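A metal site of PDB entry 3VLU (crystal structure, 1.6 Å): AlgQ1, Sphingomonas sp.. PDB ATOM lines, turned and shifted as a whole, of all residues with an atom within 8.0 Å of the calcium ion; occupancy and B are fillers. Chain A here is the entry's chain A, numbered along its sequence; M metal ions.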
ATOM      1  N   TRP A 145       5.117 -14.403   8.110  1.00  0.00           N
ATOM      2  CA  TRP A 145       6.443 -13.841   7.849  1.00  0.00           C
ATOM      3  C   TRP A 145       7.123 -14.520   6.670  1.00  0.00           C
ATOM      4  O   TRP A 145       7.776 -13.870   5.861  1.00  0.00           O
ATOM      5  CB  TRP A 145       7.306 -13.923   9.109  1.00  0.00           C
ATOM      6  CG  TRP A 145       7.012 -12.840  10.113  1.00  0.00           C
ATOM      7  CD1 TRP A 145       5.960 -11.958  10.087  1.00  0.00           C
ATOM      8  CD2 TRP A 145       7.752 -12.539  11.307  1.00  0.00           C
ATOM      9  NE1 TRP A 145       6.013 -11.123  11.171  1.00  0.00           N
ATOM     10  CE2 TRP A 145       7.100 -11.457  11.935  1.00  0.00           C
ATOM     11  CE3 TRP A 145       8.911 -13.072  11.885  1.00  0.00           C
ATOM     12  CZ2 TRP A 145       7.567 -10.901  13.128  1.00  0.00           C
ATOM     13  CZ3 TRP A 145       9.378 -12.516  13.077  1.00  0.00           C
ATOM     14  CH2 TRP A 145       8.702 -11.443  13.682  1.00  0.00           C
ATOM     15  N   PHE A 167      14.359 -13.271   8.885  1.00  0.00           N
ATOM     16  CA  PHE A 167      13.507 -12.785   9.962  1.00  0.00           C
ATOM     17  C   PHE A 167      14.212 -11.671  10.736  1.00  0.00           C
ATOM     18  O   PHE A 167      13.600 -10.646  11.053  1.00  0.00           O
ATOM     19  CB  PHE A 167      13.150 -13.938  10.926  1.00  0.00           C
ATOM     20  CG  PHE A 167      12.067 -14.861  10.424  1.00  0.00           C
ATOM     21  CD1 PHE A 167      11.547 -14.747   9.135  1.00  0.00           C
ATOM     22  CD2 PHE A 167      11.586 -15.877  11.250  1.00  0.00           C
ATOM     23  CE1 PHE A 167      10.553 -15.615   8.683  1.00  0.00           C
ATOM     24  CE2 PHE A 167      10.595 -16.744  10.812  1.00  0.00           C
ATOM     25  CZ  PHE A 167      10.069 -16.618   9.523  1.00  0.00           C
ATOM     26  N   LYS A 168      15.491 -11.873  11.028  1.00  0.00           N
ATOM     27  CA  LYS A 168      16.267 -10.890  11.785  1.00  0.00           C
ATOM     28  C   LYS A 168      16.537  -9.600  11.008  1.00  0.00           C
ATOM     29  O   LYS A 168      16.476  -8.500  11.572  1.00  0.00           O
ATOM     30  CB  LYS A 168      17.603 -11.497  12.246  1.00  0.00           C
ATOM     31  CG  LYS A 168      18.337 -10.641  13.267  1.00  0.00           C
ATOM     32  CD  LYS A 168      19.735 -11.146  13.534  1.00  0.00           C
ATOM     33  CE  LYS A 168      20.438 -10.267  14.568  1.00  0.00           C
ATOM     34  NZ  LYS A 168      20.802  -8.930  14.028  1.00  0.00           N
ATOM     35  N   GLU A 169      16.803  -9.725   9.711  1.00  0.00           N
ATOM     36  CA  GLU A 169      17.366  -8.618   8.928  1.00  0.00           C
ATOM     37  C   GLU A 169      16.398  -7.890   7.998  1.00  0.00           C
ATOM     38  O   GLU A 169      16.636  -6.726   7.663  1.00  0.00           O
ATOM     39  CB  GLU A 169      18.567  -9.126   8.107  1.00  0.00           C
ATOM     40  CG  GLU A 169      19.757  -9.587   8.942  1.00  0.00           C
ATOM     41  CD  GLU A 169      20.865 -10.216   8.105  1.00  0.00           C
ATOM     42  OE1 GLU A 169      20.640 -10.517   6.916  1.00  0.00           O
ATOM     43  OE2 GLU A 169      21.963 -10.424   8.657  1.00  0.00           O
ATOM     44  N   LYS A 170      15.320  -8.565   7.584  1.00  0.00           N
ATOM     45  CA  LYS A 170      14.449  -8.058   6.521  1.00  0.00           C
ATOM     46  C   LYS A 170      13.131  -7.455   7.022  1.00  0.00           C
ATOM     47  O   LYS A 170      12.174  -7.302   6.244  1.00  0.00           O
ATOM     48  CB  LYS A 170      14.195  -9.139   5.475  1.00  0.00           C
ATOM     49  CG  LYS A 170      15.376  -9.424   4.552  1.00  0.00           C
ATOM     50  CD  LYS A 170      15.477  -8.377   3.455  1.00  0.00           C
ATOM     51  CE  LYS A 170      15.577  -6.974   4.018  1.00  0.00           C
ATOM     52  NZ  LYS A 170      15.601  -5.942   2.947  1.00  0.00           N
ATOM     53  N   ASP A 171      13.084  -7.108   8.307  1.00  0.00           N
ATOM     54  CA  ASP A 171      11.959  -6.364   8.894  1.00  0.00           C
ATOM     55  C   ASP A 171      10.562  -6.911   8.545  1.00  0.00           C
ATOM     56  O   ASP A 171       9.727  -6.188   7.993  1.00  0.00           O
ATOM     57  CB  ASP A 171      12.094  -4.877   8.500  1.00  0.00           C
ATOM     58  CG  ASP A 171      11.097  -3.978   9.216  1.00  0.00           C
ATOM     59  OD1 ASP A 171      10.617  -3.012   8.591  1.00  0.00           O
ATOM     60  OD2 ASP A 171      10.802  -4.228  10.401  1.00  0.00           O
ATOM     61  N   PRO A 172      10.289  -8.194   8.873  1.00  0.00           N
ATOM     62  CA  PRO A 172       8.970  -8.759   8.530  1.00  0.00           C
ATOM     63  C   PRO A 172       7.781  -8.132   9.269  1.00  0.00           C
ATOM     64  O   PRO A 172       6.663  -8.227   8.774  1.00  0.00           O
ATOM     65  CB  PRO A 172       9.123 -10.242   8.894  1.00  0.00           C
ATOM     66  CG  PRO A 172      10.239 -10.291   9.869  1.00  0.00           C
ATOM     67  CD  PRO A 172      11.184  -9.219   9.443  1.00  0.00           C
ATOM     68  N   ASN A 173       8.003  -7.494  10.418  1.00  0.00           N
ATOM     69  CA  ASN A 173       6.906  -6.788  11.089  1.00  0.00           C
ATOM     70  C   ASN A 173       6.669  -5.367  10.543  1.00  0.00           C
ATOM     71  O   ASN A 173       5.691  -4.721  10.892  1.00  0.00           O
ATOM     72  CB  ASN A 173       7.016  -6.836  12.635  1.00  0.00           C
ATOM     73  CG  ASN A 173       8.150  -5.986  13.202  1.00  0.00           C
ATOM     74  OD1 ASN A 173       8.674  -5.084  12.547  1.00  0.00           O
ATOM     75  ND2 ASN A 173       8.520  -6.285  14.441  1.00  0.00           N
ATOM     76  N   GLY A 174       7.594  -4.923   9.691  1.00  0.00           N
ATOM     77  CA  GLY A 174       7.404  -3.709   8.891  1.00  0.00           C
ATOM     78  C   GLY A 174       7.434  -2.380   9.619  1.00  0.00           C
ATOM     79  O   GLY A 174       6.824  -1.414   9.161  1.00  0.00           O
ATOM     80  N   ASN A 175       8.140  -2.326  10.748  1.00  0.00           N
ATOM     81  CA  ASN A 175       8.229  -1.089  11.532  1.00  0.00           C
ATOM     82  C   ASN A 175       9.536  -0.310  11.300  1.00  0.00           C
ATOM     83  O   ASN A 175       9.784   0.703  11.966  1.00  0.00           O
ATOM     84  CB  ASN A 175       7.998  -1.358  13.023  1.00  0.00           C
ATOM     85  CG  ASN A 175       8.994  -2.344  13.618  1.00  0.00           C
ATOM     86  OD1 ASN A 175      10.004  -2.695  13.014  1.00  0.00           O
ATOM     87  ND2 ASN A 175       8.699  -2.785  14.843  1.00  0.00           N
ATOM     88  N   GLY A 176      10.341  -0.771  10.357  1.00  0.00           N
ATOM     89  CA  GLY A 176      11.616  -0.143  10.024  1.00  0.00           C
ATOM     90  C   GLY A 176      12.703  -0.304  11.070  1.00  0.00           C
ATOM     91  O   GLY A 176      13.741   0.363  11.000  1.00  0.00           O
ATOM     92  N   LYS A 177      12.470  -1.195  12.036  1.00  0.00           N
ATOM     93  CA  LYS A 177      13.416  -1.455  13.104  1.00  0.00           C
ATOM     94  C   LYS A 177      13.857  -2.916  13.119  1.00  0.00           C
ATOM     95  O   LYS A 177      13.076  -3.807  12.786  1.00  0.00           O
ATOM     96  CB  LYS A 177      12.825  -1.073  14.468  1.00  0.00           C
ATOM     97  CG  LYS A 177      12.602   0.418  14.649  1.00  0.00           C
ATOM     98  CD  LYS A 177      11.970   0.735  15.997  1.00  0.00           C
ATOM     99  CE  LYS A 177      10.593   0.109  16.113  1.00  0.00           C
ATOM    100  NZ  LYS A 177       9.956   0.418  17.426  1.00  0.00           N
ATOM    101  N   ALA A 178      15.104  -3.146  13.500  1.00  0.00           N
ATOM    102  CA  ALA A 178      15.638  -4.498  13.640  1.00  0.00           C
ATOM    103  C   ALA A 178      15.328  -5.002  15.045  1.00  0.00           C
ATOM    104  O   ALA A 178      16.223  -5.134  15.886  1.00  0.00           O
ATOM    105  CB  ALA A 178      17.140  -4.517  13.363  1.00  0.00           C
ATOM    106  N   ASP A 179      14.049  -5.275  15.280  1.00  0.00           N
ATOM    107  CA  ASP A 179      13.551  -5.675  16.592  1.00  0.00           C
ATOM    108  C   ASP A 179      13.154  -7.151  16.646  1.00  0.00           C
ATOM    109  O   ASP A 179      12.871  -7.695  17.721  1.00  0.00           O
ATOM    110  CB  ASP A 179      12.381  -4.773  17.036  1.00  0.00           C
ATOM    111  CG  ASP A 179      11.179  -4.819  16.078  1.00  0.00           C
ATOM    112  OD1 ASP A 179      10.072  -4.443  16.529  1.00  0.00           O
ATOM    113  OD2 ASP A 179      11.321  -5.213  14.898  1.00  0.00           O
ATOM    114  N   GLU A 180      13.146  -7.795  15.477  1.00  0.00           N
ATOM    115  CA  GLU A 180      12.738  -9.196  15.362  1.00  0.00           C
ATOM    116  C   GLU A 180      13.712 -10.135  16.048  1.00  0.00           C
ATOM    117  O   GLU A 180      14.925  -9.987  15.944  1.00  0.00           O
ATOM    118  CB  GLU A 180      12.591  -9.593  13.892  1.00  0.00           C
ATOM    119  CG  GLU A 180      11.348  -9.040  13.209  1.00  0.00           C
ATOM    120  CD  GLU A 180      11.505  -7.643  12.640  1.00  0.00           C
ATOM    121  OE1 GLU A 180      10.561  -7.176  11.974  1.00  0.00           O
ATOM    122  OE2 GLU A 180      12.562  -6.997  12.829  1.00  0.00           O
ATOM    123  N   ILE A 181      13.145 -11.107  16.760  1.00  0.00           N
ATOM    124  CA  ILE A 181      13.907 -12.175  17.399  1.00  0.00           C
ATOM    125  C   ILE A 181      13.452 -13.492  16.767  1.00  0.00           C
ATOM    126  O   ILE A 181      12.348 -13.959  17.052  1.00  0.00           O
ATOM    127  CB  ILE A 181      13.686 -12.207  18.933  1.00  0.00           C
ATOM    128  CG1 ILE A 181      14.007 -10.851  19.556  1.00  0.00           C
ATOM    129  CG2 ILE A 181      14.529 -13.306  19.562  1.00  0.00           C
ATOM    130  CD1 ILE A 181      13.510 -10.678  20.982  1.00  0.00           C
ATOM    131  N   ASN A 261       4.110  -8.758  20.891  1.00  0.00           N
ATOM    132  CA  ASN A 261       4.716  -7.549  20.339  1.00  0.00           C
ATOM    133  C   ASN A 261       5.176  -7.730  18.886  1.00  0.00           C
ATOM    134  O   ASN A 261       5.816  -6.840  18.306  1.00  0.00           O
ATOM    135  CB  ASN A 261       5.876  -7.072  21.232  1.00  0.00           C
ATOM    136  CG  ASN A 261       6.363  -5.672  20.893  1.00  0.00           C
ATOM    137  OD1 ASN A 261       7.563  -5.397  20.931  1.00  0.00           O
ATOM    138  ND2 ASN A 261       5.444  -4.781  20.554  1.00  0.00           N
ATOM    139  N   ASN A 262       4.836  -8.878  18.313  1.00  0.00           N
ATOM    140  CA  ASN A 262       5.135  -9.201  16.904  1.00  0.00           C
ATOM    141  C   ASN A 262       6.633  -9.172  16.568  1.00  0.00           C
ATOM    142  O   ASN A 262       7.042  -8.625  15.544  1.00  0.00           O
ATOM    143  CB  ASN A 262       4.314  -8.285  15.967  1.00  0.00           C
ATOM    144  CG  ASN A 262       4.242  -8.814  14.538  1.00  0.00           C
ATOM    145  OD1 ASN A 262       4.543  -9.972  14.270  1.00  0.00           O
ATOM    146  ND2 ASN A 262       3.827  -7.950  13.620  1.00  0.00           N
ATOM    147  N   ILE A 263       7.440  -9.761  17.446  1.00  0.00           N
ATOM    148  CA  ILE A 263       8.881  -9.843  17.216  1.00  0.00           C
ATOM    149  C   ILE A 263       9.420 -11.282  17.119  1.00  0.00           C
ATOM    150  O   ILE A 263      10.499 -11.503  16.587  1.00  0.00           O
ATOM    151  CB  ILE A 263       9.708  -8.998  18.223  1.00  0.00           C
ATOM    152  CG1 ILE A 263       9.350  -9.355  19.675  1.00  0.00           C
ATOM    153  CG2 ILE A 263       9.514  -7.501  17.947  1.00  0.00           C
ATOM    154  CD1 ILE A 263      10.241  -8.709  20.730  1.00  0.00           C
HETATM  155 CA    CA M   1      10.976  -4.776  12.636  1.00  0.00          CA
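N of Gly 174 sits close to OD2 of Asp 171, 3.4 Å away. OD1 of Asp 171 lies within hydrogen-bond range of N of Gly 176 (2.9 Å). The backbone carbonyl oxygen of Asn 262 sits at hydrogen-bond distance from the side-chain amide nitrogen of Asn 173 (3.0 Å).
The nearest printed residue that does not touch the calcium ion is Gly 174 (4.5 Å).
The calcium ion is bound by the side-chain carboxylate (OD2) of Asp 171. O of Lys 177 binds the calcium ion, at 2.3 Å. The calcium ion is bound by OD1 of Asn 173, 2.3 Å away. OD1 of Asn 175 binds the calcium ion (2.3 Å). The side-chain carboxylate (OD2) of Asp 179 binds the calcium ion, at 2.3 Å. OE1 of Glu 180 is bound to the calcium ion, at 2.5 Å. The calcium ion is bound by the side-chain carboxylate (OE2) of Glu 180. The calcium ion has seven donor atoms within binding distance.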
